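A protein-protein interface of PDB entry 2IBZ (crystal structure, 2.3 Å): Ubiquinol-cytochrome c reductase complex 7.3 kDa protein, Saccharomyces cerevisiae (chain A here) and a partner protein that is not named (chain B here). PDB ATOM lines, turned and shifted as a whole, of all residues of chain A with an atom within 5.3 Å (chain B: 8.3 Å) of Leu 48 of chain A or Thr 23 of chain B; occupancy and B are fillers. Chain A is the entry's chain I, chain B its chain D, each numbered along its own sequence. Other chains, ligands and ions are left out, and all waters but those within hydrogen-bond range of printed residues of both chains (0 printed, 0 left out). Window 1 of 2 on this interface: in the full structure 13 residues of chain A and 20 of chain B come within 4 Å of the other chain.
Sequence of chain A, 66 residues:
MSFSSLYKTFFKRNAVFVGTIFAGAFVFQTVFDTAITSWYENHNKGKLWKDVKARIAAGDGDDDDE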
ATOM      1  N   TYR A  40       7.034 -35.429  -6.084  1.00  0.00           N
ATOM      2  CA  TYR A  40       6.833 -34.082  -5.560  1.00  0.00           C
ATOM      3  C   TYR A  40       7.598 -33.018  -6.345  1.00  0.00           C
ATOM      4  O   TYR A  40       7.015 -32.009  -6.748  1.00  0.00           O
ATOM      5  CB  TYR A  40       7.222 -34.039  -4.075  1.00  0.00           C
ATOM      6  CG  TYR A  40       6.785 -32.802  -3.322  1.00  0.00           C
ATOM      7  CD1 TYR A  40       5.435 -32.585  -3.011  1.00  0.00           C
ATOM      8  CD2 TYR A  40       7.726 -31.878  -2.865  1.00  0.00           C
ATOM      9  CE1 TYR A  40       5.038 -31.480  -2.259  1.00  0.00           C
ATOM     10  CE2 TYR A  40       7.341 -30.771  -2.112  1.00  0.00           C
ATOM     11  CZ  TYR A  40       5.999 -30.578  -1.816  1.00  0.00           C
ATOM     12  OH  TYR A  40       5.632 -29.478  -1.087  1.00  0.00           O
ATOM     13  N   GLU A  41       8.896 -33.234  -6.548  1.00  0.00           N
ATOM     14  CA  GLU A  41       9.716 -32.271  -7.286  1.00  0.00           C
ATOM     15  C   GLU A  41       9.293 -32.130  -8.754  1.00  0.00           C
ATOM     16  O   GLU A  41       9.358 -31.041  -9.324  1.00  0.00           O
ATOM     17  CB  GLU A  41      11.198 -32.632  -7.196  1.00  0.00           C
ATOM     18  CG  GLU A  41      11.785 -32.433  -5.825  1.00  0.00           C
ATOM     19  CD  GLU A  41      13.300 -32.461  -5.826  1.00  0.00           C
ATOM     20  OE1 GLU A  41      13.894 -31.773  -4.966  1.00  0.00           O
ATOM     21  OE2 GLU A  41      13.900 -33.167  -6.676  1.00  0.00           O
ATOM     22  N   ASN A  44       6.080 -30.175  -9.114  1.00  0.00           N
ATOM     23  CA  ASN A  44       6.346 -28.750  -8.919  1.00  0.00           C
ATOM     24  C   ASN A  44       7.441 -28.156  -9.805  1.00  0.00           C
ATOM     25  O   ASN A  44       8.024 -27.119  -9.477  1.00  0.00           O
ATOM     26  CB  ASN A  44       6.657 -28.469  -7.448  1.00  0.00           C
ATOM     27  CG  ASN A  44       5.409 -28.414  -6.601  1.00  0.00           C
ATOM     28  OD1 ASN A  44       4.787 -27.361  -6.475  1.00  0.00           O
ATOM     29  ND2 ASN A  44       5.019 -29.554  -6.039  1.00  0.00           N
ATOM     30  N   LYS A  45       7.690 -28.801 -10.943  1.00  0.00           N
ATOM     31  CA  LYS A  45       8.703 -28.356 -11.893  1.00  0.00           C
ATOM     32  C   LYS A  45       8.423 -26.914 -12.333  1.00  0.00           C
ATOM     33  O   LYS A  45       7.285 -26.552 -12.626  1.00  0.00           O
ATOM     34  CB  LYS A  45       8.716 -29.290 -13.108  1.00  0.00           C
ATOM     35  CG  LYS A  45      10.013 -29.272 -13.901  1.00  0.00           C
ATOM     36  CD  LYS A  45       9.860 -30.031 -15.223  1.00  0.00           C
ATOM     37  CE  LYS A  45       9.628 -31.532 -15.018  1.00  0.00           C
ATOM     38  NZ  LYS A  45      10.812 -32.222 -14.408  1.00  0.00           N
ATOM     39  N   GLY A  46       9.462 -26.090 -12.319  1.00  0.00           N
ATOM     40  CA  GLY A  46       9.318 -24.700 -12.702  1.00  0.00           C
ATOM     41  C   GLY A  46       9.276 -23.751 -11.523  1.00  0.00           C
ATOM     42  O   GLY A  46       9.750 -22.619 -11.621  1.00  0.00           O
ATOM     43  N   LYS A  47       8.746 -24.227 -10.394  1.00  0.00           N
ATOM     44  CA  LYS A  47       8.610 -23.421  -9.184  1.00  0.00           C
ATOM     45  C   LYS A  47       9.768 -23.540  -8.216  1.00  0.00           C
ATOM     46  O   LYS A  47      10.028 -22.616  -7.443  1.00  0.00           O
ATOM     47  CB  LYS A  47       7.311 -23.787  -8.477  1.00  0.00           C
ATOM     48  CG  LYS A  47       6.069 -23.374  -9.238  1.00  0.00           C
ATOM     49  CD  LYS A  47       4.900 -24.323  -8.996  1.00  0.00           C
ATOM     50  CE  LYS A  47       4.409 -24.294  -7.567  1.00  0.00           C
ATOM     51  NZ  LYS A  47       3.296 -25.260  -7.374  1.00  0.00           N
ATOM     52  N   LEU A  48      10.457 -24.678  -8.260  1.00  0.00           N
ATOM     53  CA  LEU A  48      11.597 -24.954  -7.377  1.00  0.00           C
ATOM     54  C   LEU A  48      12.792 -24.028  -7.548  1.00  0.00           C
ATOM     55  O   LEU A  48      12.964 -23.395  -8.592  1.00  0.00           O
ATOM     56  CB  LEU A  48      12.073 -26.393  -7.571  1.00  0.00           C
ATOM     57  CG  LEU A  48      11.416 -27.541  -6.801  1.00  0.00           C
ATOM     58  CD1 LEU A  48      10.054 -27.138  -6.241  1.00  0.00           C
ATOM     59  CD2 LEU A  48      11.312 -28.764  -7.710  1.00  0.00           C
ATOM     60  N   TRP A  49      13.615 -23.947  -6.509  1.00  0.00           N
ATOM     61  CA  TRP A  49      14.822 -23.129  -6.561  1.00  0.00           C
ATOM     62  C   TRP A  49      15.810 -23.706  -7.592  1.00  0.00           C
ATOM     63  O   TRP A  49      16.572 -22.962  -8.200  1.00  0.00           O
ATOM     64  CB  TRP A  49      15.485 -23.055  -5.184  1.00  0.00           C
ATOM     65  CG  TRP A  49      16.862 -22.473  -5.221  1.00  0.00           C
ATOM     66  CD1 TRP A  49      18.026 -23.093  -4.863  1.00  0.00           C
ATOM     67  CD2 TRP A  49      17.224 -21.151  -5.647  1.00  0.00           C
ATOM     68  NE1 TRP A  49      19.090 -22.238  -5.036  1.00  0.00           N
ATOM     69  CE2 TRP A  49      18.626 -21.041  -5.513  1.00  0.00           C
ATOM     70  CE3 TRP A  49      16.499 -20.053  -6.129  1.00  0.00           C
ATOM     71  CZ2 TRP A  49      19.319 -19.872  -5.842  1.00  0.00           C
ATOM     72  CZ3 TRP A  49      17.187 -18.891  -6.456  1.00  0.00           C
ATOM     73  CH2 TRP A  49      18.584 -18.810  -6.310  1.00  0.00           C
ATOM     74  N   LYS A  50      15.798 -25.030  -7.768  1.00  0.00           N
ATOM     75  CA  LYS A  50      16.670 -25.704  -8.736  1.00  0.00           C
ATOM     76  C   LYS A  50      16.409 -25.108 -10.106  1.00  0.00           C
ATOM     77  O   LYS A  50      17.336 -24.785 -10.845  1.00  0.00           O
ATOM     78  CB  LYS A  50      16.347 -27.198  -8.842  1.00  0.00           C
ATOM     79  CG  LYS A  50      16.497 -28.024  -7.580  1.00  0.00           C
ATOM     80  CD  LYS A  50      16.396 -29.520  -7.905  1.00  0.00           C
ATOM     81  CE  LYS A  50      15.150 -29.851  -8.738  1.00  0.00           C
ATOM     82  NZ  LYS A  50      15.028 -31.313  -9.057  1.00  0.00           N
ATOM     83  N   ASP A  51      15.126 -24.984 -10.428  1.00  0.00           N
ATOM     84  CA  ASP A  51      14.673 -24.453 -11.702  1.00  0.00           C
ATOM     85  C   ASP A  51      14.983 -22.975 -11.858  1.00  0.00           C
ATOM     86  O   ASP A  51      15.377 -22.532 -12.933  1.00  0.00           O
ATOM     87  CB  ASP A  51      13.176 -24.715 -11.866  1.00  0.00           C
ATOM     88  CG  ASP A  51      12.809 -26.174 -11.612  1.00  0.00           C
ATOM     89  OD1 ASP A  51      11.703 -26.433 -11.096  1.00  0.00           O
ATOM     90  OD2 ASP A  51      13.632 -27.068 -11.909  1.00  0.00           O
ATOM     91  N   VAL A  52      14.831 -22.217 -10.782  1.00  0.00           N
ATOM     92  CA  VAL A  52      15.105 -20.786 -10.825  1.00  0.00           C
ATOM     93  C   VAL A  52      16.599 -20.511 -10.995  1.00  0.00           C
ATOM     94  O   VAL A  52      16.982 -19.574 -11.701  1.00  0.00           O
ATOM     95  CB  VAL A  52      14.582 -20.076  -9.556  1.00  0.00           C
ATOM     96  CG1 VAL A  52      14.856 -18.584  -9.625  1.00  0.00           C
ATOM     97  CG2 VAL A  52      13.094 -20.330  -9.401  1.00  0.00           C
ATOM     98  N   LYS A  53      17.437 -21.348 -10.385  1.00  0.00           N
ATOM     99  CA  LYS A  53      18.886 -21.179 -10.472  1.00  0.00           C
ATOM    100  C   LYS A  53      19.417 -21.427 -11.886  1.00  0.00           C
ATOM    101  O   LYS A  53      20.443 -20.865 -12.278  1.00  0.00           O
ATOM    102  CB  LYS A  53      19.605 -22.089  -9.473  1.00  0.00           C
ATOM    103  CG  LYS A  53      21.071 -21.719  -9.288  1.00  0.00           C
ATOM    104  CD  LYS A  53      21.797 -22.626  -8.306  1.00  0.00           C
ATOM    105  CE  LYS A  53      23.241 -22.158  -8.117  1.00  0.00           C
ATOM    106  NZ  LYS A  53      24.007 -22.981  -7.135  1.00  0.00           N
ATOM    107  N   TRP B  15      -3.553 -18.661  -5.850  1.00  0.00           N
ATOM    108  CA  TRP B  15      -2.141 -18.710  -5.516  1.00  0.00           C
ATOM    109  C   TRP B  15      -1.596 -20.044  -5.961  1.00  0.00           C
ATOM    110  O   TRP B  15      -2.276 -21.061  -5.831  1.00  0.00           O
ATOM    111  CB  TRP B  15      -1.935 -18.513  -4.027  1.00  0.00           C
ATOM    112  CG  TRP B  15      -2.427 -17.210  -3.559  1.00  0.00           C
ATOM    113  CD1 TRP B  15      -3.652 -16.945  -3.046  1.00  0.00           C
ATOM    114  CD2 TRP B  15      -1.718 -15.973  -3.573  1.00  0.00           C
ATOM    115  NE1 TRP B  15      -3.760 -15.610  -2.734  1.00  0.00           N
ATOM    116  CE2 TRP B  15      -2.585 -14.988  -3.050  1.00  0.00           C
ATOM    117  CE3 TRP B  15      -0.433 -15.594  -3.981  1.00  0.00           C
ATOM    118  CZ2 TRP B  15      -2.213 -13.646  -2.925  1.00  0.00           C
ATOM    119  CZ3 TRP B  15      -0.062 -14.254  -3.857  1.00  0.00           C
ATOM    120  CH2 TRP B  15      -0.950 -13.300  -3.334  1.00  0.00           C
ATOM    121  N   SER B  16      -0.393 -20.028  -6.536  1.00  0.00           N
ATOM    122  CA  SER B  16       0.217 -21.251  -7.037  1.00  0.00           C
ATOM    123  C   SER B  16       0.605 -22.204  -5.900  1.00  0.00           C
ATOM    124  O   SER B  16       0.744 -23.415  -6.119  1.00  0.00           O
ATOM    125  CB  SER B  16       1.398 -20.944  -7.977  1.00  0.00           C
ATOM    126  OG  SER B  16       2.330 -20.046  -7.396  1.00  0.00           O
ATOM    127  N   HIS B  17       0.762 -21.660  -4.689  1.00  0.00           N
ATOM    128  CA  HIS B  17       1.080 -22.493  -3.530  1.00  0.00           C
ATOM    129  C   HIS B  17      -0.141 -23.099  -2.816  1.00  0.00           C
ATOM    130  O   HIS B  17       0.023 -23.868  -1.870  1.00  0.00           O
ATOM    131  CB  HIS B  17       2.006 -21.776  -2.540  1.00  0.00           C
ATOM    132  CG  HIS B  17       1.600 -20.376  -2.209  1.00  0.00           C
ATOM    133  ND1 HIS B  17       0.938 -20.050  -1.044  1.00  0.00           N
ATOM    134  CD2 HIS B  17       1.846 -19.203  -2.840  1.00  0.00           C
ATOM    135  CE1 HIS B  17       0.802 -18.738  -0.968  1.00  0.00           C
ATOM    136  NE2 HIS B  17       1.345 -18.201  -2.044  1.00  0.00           N
ATOM    137  N   ASN B  18      -1.356 -22.742  -3.254  1.00  0.00           N
ATOM    138  CA  ASN B  18      -2.587 -23.294  -2.670  1.00  0.00           C
ATOM    139  C   ASN B  18      -2.671 -24.720  -3.194  1.00  0.00           C
ATOM    140  O   ASN B  18      -2.378 -24.963  -4.373  1.00  0.00           O
ATOM    141  CB  ASN B  18      -3.844 -22.553  -3.155  1.00  0.00           C
ATOM    142  CG  ASN B  18      -4.090 -21.243  -2.438  1.00  0.00           C
ATOM    143  OD1 ASN B  18      -5.037 -20.533  -2.768  1.00  0.00           O
ATOM    144  ND2 ASN B  18      -3.266 -20.921  -1.451  1.00  0.00           N
ATOM    145  N   GLY B  19      -3.116 -25.649  -2.358  1.00  0.00           N
ATOM    146  CA  GLY B  19      -3.199 -27.025  -2.810  1.00  0.00           C
ATOM    147  C   GLY B  19      -2.226 -27.856  -2.009  1.00  0.00           C
ATOM    148  O   GLY B  19      -1.100 -27.425  -1.760  1.00  0.00           O
ATOM    149  N   PRO B  20      -2.626 -29.068  -1.603  1.00  0.00           N
ATOM    150  CA  PRO B  20      -1.780 -29.968  -0.810  1.00  0.00           C
ATOM    151  C   PRO B  20      -0.455 -30.377  -1.439  1.00  0.00           C
ATOM    152  O   PRO B  20       0.549 -30.539  -0.728  1.00  0.00           O
ATOM    153  CB  PRO B  20      -2.699 -31.167  -0.545  1.00  0.00           C
ATOM    154  CG  PRO B  20      -3.647 -31.142  -1.710  1.00  0.00           C
ATOM    155  CD  PRO B  20      -3.931 -29.681  -1.898  1.00  0.00           C
ATOM    156  N   PHE B  21      -0.435 -30.481  -2.766  1.00  0.00           N
ATOM    157  CA  PHE B  21       0.772 -30.892  -3.475  1.00  0.00           C
ATOM    158  C   PHE B  21       1.628 -29.740  -3.984  1.00  0.00           C
ATOM    159  O   PHE B  21       2.689 -29.977  -4.532  1.00  0.00           O
ATOM    160  CB  PHE B  21       0.414 -31.795  -4.657  1.00  0.00           C
ATOM    161  CG  PHE B  21      -0.555 -32.899  -4.318  1.00  0.00           C
ATOM    162  CD1 PHE B  21      -1.746 -33.031  -5.021  1.00  0.00           C
ATOM    163  CD2 PHE B  21      -0.275 -33.805  -3.307  1.00  0.00           C
ATOM    164  CE1 PHE B  21      -2.652 -34.054  -4.717  1.00  0.00           C
ATOM    165  CE2 PHE B  21      -1.172 -34.829  -2.996  1.00  0.00           C
ATOM    166  CZ  PHE B  21      -2.360 -34.955  -3.701  1.00  0.00           C
ATOM    167  N   GLU B  22       1.228 -28.502  -3.710  1.00  0.00           N
ATOM    168  CA  GLU B  22       1.955 -27.334  -4.223  1.00  0.00           C
ATOM    169  C   GLU B  22       3.012 -26.635  -3.376  1.00  0.00           C
ATOM    170  O   GLU B  22       2.738 -26.216  -2.252  1.00  0.00           O
ATOM    171  CB  GLU B  22       0.948 -26.282  -4.684  1.00  0.00           C
ATOM    172  CG  GLU B  22      -0.192 -26.843  -5.519  1.00  0.00           C
ATOM    173  CD  GLU B  22       0.296 -27.577  -6.752  1.00  0.00           C
ATOM    174  OE1 GLU B  22      -0.289 -28.628  -7.090  1.00  0.00           O
ATOM    175  OE2 GLU B  22       1.268 -27.101  -7.377  1.00  0.00           O
ATOM    176  N   THR B  23       4.193 -26.434  -3.955  1.00  0.00           N
ATOM    177  CA  THR B  23       5.279 -25.726  -3.274  1.00  0.00           C
ATOM    178  C   THR B  23       5.136 -24.242  -3.592  1.00  0.00           C
ATOM    179  O   THR B  23       4.309 -23.856  -4.410  1.00  0.00           O
ATOM    180  CB  THR B  23       6.679 -26.138  -3.800  1.00  0.00           C
ATOM    181  OG1 THR B  23       6.808 -25.755  -5.181  1.00  0.00           O
ATOM    182  CG2 THR B  23       6.897 -27.635  -3.658  1.00  0.00           C
ATOM    183  N   PHE B  24       5.927 -23.404  -2.940  1.00  0.00           N
ATOM    184  CA  PHE B  24       5.902 -21.989  -3.263  1.00  0.00           C
ATOM    185  C   PHE B  24       6.542 -21.868  -4.656  1.00  0.00           C
ATOM    186  O   PHE B  24       7.226 -22.791  -5.123  1.00  0.00           O
ATOM    187  CB  PHE B  24       6.804 -21.188  -2.320  1.00  0.00           C
ATOM    188  CG  PHE B  24       6.208 -20.901  -0.983  1.00  0.00           C
ATOM    189  CD1 PHE B  24       6.973 -21.067   0.174  1.00  0.00           C
ATOM    190  CD2 PHE B  24       4.921 -20.404  -0.868  1.00  0.00           C
ATOM    191  CE1 PHE B  24       6.462 -20.733   1.419  1.00  0.00           C
ATOM    192  CE2 PHE B  24       4.401 -20.068   0.382  1.00  0.00           C
ATOM    193  CZ  PHE B  24       5.174 -20.232   1.519  1.00  0.00           C
ATOM    194  N   ASP B  25       6.312 -20.736  -5.312  1.00  0.00           N
ATOM    195  CA  ASP B  25       6.941 -20.463  -6.593  1.00  0.00           C
ATOM    196  C   ASP B  25       8.138 -19.626  -6.153  1.00  0.00           C
ATOM    197  O   ASP B  25       7.978 -18.478  -5.735  1.00  0.00           O
ATOM    198  CB  ASP B  25       6.023 -19.635  -7.488  1.00  0.00           C
ATOM    199  CG  ASP B  25       6.611 -19.391  -8.871  1.00  0.00           C
ATOM    200  OD1 ASP B  25       5.980 -19.826  -9.856  1.00  0.00           O
ATOM    201  OD2 ASP B  25       7.687 -18.760  -8.979  1.00  0.00           O
ATOM    202  N   HIS B  26       9.330 -20.204  -6.236  1.00  0.00           N
ATOM    203  CA  HIS B  26      10.542 -19.519  -5.800  1.00  0.00           C
ATOM    204  C   HIS B  26      11.004 -18.288  -6.571  1.00  0.00           C
ATOM    205  O   HIS B  26      11.709 -17.442  -6.012  1.00  0.00           O
ATOM    206  CB  HIS B  26      11.666 -20.527  -5.603  1.00  0.00           C
ATOM    207  CG  HIS B  26      11.421 -21.459  -4.458  1.00  0.00           C
ATOM    208  ND1 HIS B  26      12.104 -21.368  -3.264  1.00  0.00           N
ATOM    209  CD2 HIS B  26      10.526 -22.463  -4.303  1.00  0.00           C
ATOM    210  CE1 HIS B  26      11.638 -22.274  -2.424  1.00  0.00           C
ATOM    211  NE2 HIS B  26      10.680 -22.950  -3.030  1.00  0.00           N
ATOM    212  N   ALA B  27      10.603 -18.174  -7.838  1.00  0.00           N
ATOM    213  CA  ALA B  27      10.949 -16.998  -8.640  1.00  0.00           C
ATOM    214  C   ALA B  27      10.149 -15.823  -8.066  1.00  0.00           C
ATOM    215  O   ALA B  27      10.667 -14.712  -7.905  1.00  0.00           O
ATOM    216  CB  ALA B  27      10.591 -17.224 -10.103  1.00  0.00           C
ATOM    217  N   ILE B  29       9.177 -15.612  -5.039  1.00  0.00           N
ATOM    218  CA  ILE B  29       9.771 -15.274  -3.747  1.00  0.00           C
ATOM    219  C   ILE B  29      10.944 -14.339  -4.000  1.00  0.00           C
ATOM    220  O   ILE B  29      11.071 -13.304  -3.339  1.00  0.00           O
ATOM    221  CB  ILE B  29      10.268 -16.509  -2.955  1.00  0.00           C
ATOM    222  CG1 ILE B  29       9.104 -17.450  -2.629  1.00  0.00           C
ATOM    223  CG2 ILE B  29      10.962 -16.060  -1.679  1.00  0.00           C
ATOM    224  CD1 ILE B  29       9.535 -18.688  -1.858  1.00  0.00           C
ATOM    225  N   GLY B  56      19.516 -20.728  -1.078  1.00  0.00           N
ATOM    226  CA  GLY B  56      18.895 -21.952  -1.540  1.00  0.00           C
ATOM    227  C   GLY B  56      17.395 -21.836  -1.647  1.00  0.00           C
ATOM    228  O   GLY B  56      16.719 -22.810  -2.003  1.00  0.00           O
ATOM    229  N   VAL B  57      16.865 -20.661  -1.305  1.00  0.00           N
ATOM    230  CA  VAL B  57      15.428 -20.438  -1.383  1.00  0.00           C
ATOM    231  C   VAL B  57      15.100 -19.489  -2.517  1.00  0.00           C
ATOM    232  O   VAL B  57      14.333 -19.831  -3.422  1.00  0.00           O
ATOM    233  CB  VAL B  57      14.843 -19.852  -0.063  1.00  0.00           C
ATOM    234  CG1 VAL B  57      13.356 -19.517  -0.249  1.00  0.00           C
ATOM    235  CG2 VAL B  57      15.024 -20.844   1.080  1.00  0.00           C
ATOM    236  N   SER B  58      15.694 -18.302  -2.462  1.00  0.00           N
ATOM    237  CA  SER B  58      15.459 -17.272  -3.459  1.00  0.00           C
ATOM    238  C   SER B  58      16.752 -16.668  -4.020  1.00  0.00           C
ATOM    239  O   SER B  58      16.736 -16.019  -5.058  1.00  0.00           O
ATOM    240  CB  SER B  58      14.605 -16.168  -2.839  1.00  0.00           C
ATOM    241  OG  SER B  58      15.237 -15.635  -1.693  1.00  0.00           O
ATOM    242  N   THR B 192       3.827 -13.334  -1.796  1.00  0.00           N
ATOM    243  CA  THR B 192       4.353 -14.696  -1.840  1.00  0.00           C
ATOM    244  C   THR B 192       5.612 -14.749  -0.966  1.00  0.00           C
ATOM    245  O   THR B 192       5.820 -15.700  -0.200  1.00  0.00           O
ATOM    246  CB  THR B 192       4.690 -15.129  -3.283  1.00  0.00           C
ATOM    247  OG1 THR B 192       3.506 -15.055  -4.080  1.00  0.00           O
ATOM    248  CG2 THR B 192       5.181 -16.565  -3.323  1.00  0.00           C
ATOM    249  N   HIS B 202       7.105 -24.432   4.752  1.00  0.00           N
ATOM    250  CA  HIS B 202       6.032 -24.766   3.811  1.00  0.00           C
ATOM    251  C   HIS B 202       6.260 -25.922   2.816  1.00  0.00           C
ATOM    252  O   HIS B 202       5.544 -26.929   2.862  1.00  0.00           O
ATOM    253  CB  HIS B 202       5.613 -23.488   3.062  1.00  0.00           C
ATOM    254  CG  HIS B 202       4.526 -23.684   2.049  1.00  0.00           C
ATOM    255  ND1 HIS B 202       4.783 -23.941   0.718  1.00  0.00           N
ATOM    256  CD2 HIS B 202       3.177 -23.645   2.167  1.00  0.00           C
ATOM    257  CE1 HIS B 202       3.642 -24.059   0.060  1.00  0.00           C
ATOM    258  NE2 HIS B 202       2.651 -23.884   0.916  1.00  0.00           N
ATOM    259  N   ASP B 203       7.263 -25.798   1.947  1.00  0.00           N
ATOM    260  CA  ASP B 203       7.519 -26.826   0.925  1.00  0.00           C
ATOM    261  C   ASP B 203       7.840 -28.191   1.495  1.00  0.00           C
ATOM    262  O   ASP B 203       7.302 -29.206   1.055  1.00  0.00           O
ATOM    263  CB  ASP B 203       8.642 -26.382  -0.017  1.00  0.00           C
ATOM    264  CG  ASP B 203       8.289 -25.128  -0.800  1.00  0.00           C
ATOM    265  OD1 ASP B 203       7.111 -24.709  -0.805  1.00  0.00           O
ATOM    266  OD2 ASP B 203       9.203 -24.551  -1.414  1.00  0.00           O
ATOM    267  N   GLU B 204       8.737 -28.198   2.472  1.00  0.00           N
ATOM    268  CA  GLU B 204       9.151 -29.410   3.153  1.00  0.00           C
ATOM    269  C   GLU B 204       8.010 -29.984   4.000  1.00  0.00           C
ATOM    270  O   GLU B 204       7.804 -31.204   4.015  1.00  0.00           O
ATOM    271  CB  GLU B 204      10.385 -29.114   4.009  1.00  0.00           C
ATOM    272  CG  GLU B 204      10.937 -30.291   4.765  1.00  0.00           C
ATOM    273  CD  GLU B 204      11.361 -31.485   3.885  1.00  0.00           C
ATOM    274  OE1 GLU B 204      11.828 -32.488   4.473  1.00  0.00           O
ATOM    275  OE2 GLU B 204      11.232 -31.450   2.636  1.00  0.00           O
ATOM    276  N   LYS B 206       4.770 -29.911   3.505  1.00  0.00           N
ATOM    277  CA  LYS B 206       3.799 -30.603   2.661  1.00  0.00           C
ATOM    278  C   LYS B 206       4.321 -31.910   2.073  1.00  0.00           C
ATOM    279  O   LYS B 206       3.550 -32.816   1.764  1.00  0.00           O
ATOM    280  CB  LYS B 206       3.339 -29.703   1.527  1.00  0.00           C
ATOM    281  CG  LYS B 206       2.573 -28.466   1.952  1.00  0.00           C
ATOM    282  CD  LYS B 206       1.688 -28.036   0.812  1.00  0.00           C
ATOM    283  CE  LYS B 206       1.241 -26.623   0.975  1.00  0.00           C
ATOM    284  NZ  LYS B 206       0.449 -26.213  -0.207  1.00  0.00           N
ATOM    285  N   ARG B 207       5.631 -31.977   1.866  1.00  0.00           N
ATOM    286  CA  ARG B 207       6.261 -33.172   1.325  1.00  0.00           C
ATOM    287  C   ARG B 207       6.174 -34.273   2.397  1.00  0.00           C
ATOM    288  O   ARG B 207       5.845 -35.426   2.098  1.00  0.00           O
ATOM    289  CB  ARG B 207       7.717 -32.857   0.981  1.00  0.00           C
ATOM    290  CG  ARG B 207       8.391 -33.872   0.094  1.00  0.00           C
ATOM    291  CD  ARG B 207       9.904 -33.768   0.230  1.00  0.00           C
ATOM    292  NE  ARG B 207      10.397 -35.044   0.710  1.00  0.00           N
ATOM    293  CZ  ARG B 207      11.138 -35.214   1.794  1.00  0.00           C
ATOM    294  NH1 ARG B 207      11.504 -36.437   2.141  1.00  0.00           N
ATOM    295  NH2 ARG B 207      11.554 -34.174   2.498  1.00  0.00           N
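The backbone NH (N) of His 26 of chain B sits at hydrogen-bond distance from the backbone carbonyl oxygen (O) of Lys 47 of chain A (2.8 Å).
The backbone carbonyl oxygen (O) of Phe 21 of chain B is in hydrogen-bond range of the side-chain amide nitrogen (ND2) of Asn 44 of chain A.
The backbone carbonyl oxygen (O) of Ser 16 of chain B sits at hydrogen-bond distance from the side-chain amino group (NZ) of Lys 47 of chain A (3.4 Å).
The backbone NH (N) of Thr 23 of chain B sits at hydrogen-bond distance from the side-chain amide oxygen (OD1) of Asn 44 of chain A, at 2.8 Å.
The side-chain hydroxyl (OH) of Tyr 40 of chain A sits at hydrogen-bond distance from the backbone carbonyl oxygen (O) of Asp 203 of chain B.
OE2 of Glu 22 of chain B is in salt-bridge range of NZ of Lys 47 of chain A.
The side-chain amino group of Lys 47 of chain A sits close to the backbone carbonyl oxygen of Thr 23 of chain B (3.4 Å).
Leu 48 of chain A touches just one residue of chain B: Thr 23.
Of chain A, only Tyr 40 (3.4 Å), Asn 44 (2.8 Å), Lys 47 (3.2 Å) and Leu 48 (3.7 Å) come within 4 Å of Thr 23 of chain B.
Printed residues of chain A within 4 Å of Phe 21 of chain B: Tyr 40 (3.6 Å) and Asn 44 (2.8 Å).
Printed residues of chain B within 4 Å of Val 52 of chain A: Ala 27.
Of the printed residues of chain B, Trp 49 of chain A touches His 26 (3.9 Å), Gly 56 (3.2 Å), Val 57 (3.5 Å) and Ser 58 (3.2 Å).
Printed residues of chain A within 4 Å of Ser 58 of chain B: Trp 49.
The nearest residue of chain B that does not touch Leu 48 of chain A is His 26 of chain B (4.1 Å).
The nearest printed residue of chain A that does not touch Thr 23 of chain B is Glu 41 of chain A (6.5 Å).
The nearest printed residue of chain A that does not touch His 26 of chain B is Val 52 of chain A (4.1 Å).
O of Gly 19 of chain B sits at hydrogen-bond distance from NZ of Lys 206 of chain B (2.5 Å).
The side-chain carboxylate (OD2) of Asp 25 of chain B lies within hydrogen-bond range of the backbone NH (N) of Ala 27 of chain B, at 3.2 Å.
The side-chain carboxylate (OD2) of Asp 203 of chain B sits at hydrogen-bond distance from a ring nitrogen (NE2) of His 26 of chain B (2.7 Å).
The side-chain amino group (NZ) of Lys 206 of chain B lies within hydrogen-bond range of the backbone carbonyl oxygen (O) of His 17 of chain B.
NE2 of His 202 of chain B sits close to NZ of Lys 206 of chain B (3.4 Å).
ND1 of His 202 of chain B is in hydrogen-bond range of OD1 of Asp 203 of chain B, at 2.9 Å.
Of the 23 printed residues of chain B, 14 touch a printed residue of chain A.
Along chain B the printed residues that touch a printed residue of chain A span positions 16 to 207.
Hydrophobic or aromatic side chains of chain A within 4 Å of the printed part of chain B: Tyr 40, Leu 48, Trp 49 and Val 52.
Among the printed residues, 20 pairs touch across the chains.
Tyr 40 of chain A touches Phe 21 of chain B (CE1 to O, 3.6 Å).
OH of Tyr 40 of chain A touches CG2 of Thr 23 of chain B, 3.4 Å away.
Tyr 40 of chain A touches Lys 206 of chain B.
Tyr 40 of chain A touches Arg 207 of chain B (CD2 to CG, 3.6 Å).
Thr 23 of chain B touches Leu 48 of chain A.
Trp 49 of chain A touches His 26 of chain B.
Trp 49 of chain A touches Gly 56 of chain B.
CE3 of Trp 49 of chain A touches O of Val 57 of chain B, 3.5 Å away.
Ser 58 of chain B touches Trp 49 of chain A (O to CZ3, 3.2 Å).
N of Ala 27 of chain B touches CG2 of Val 52 of chain A, at 3.6 Å.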
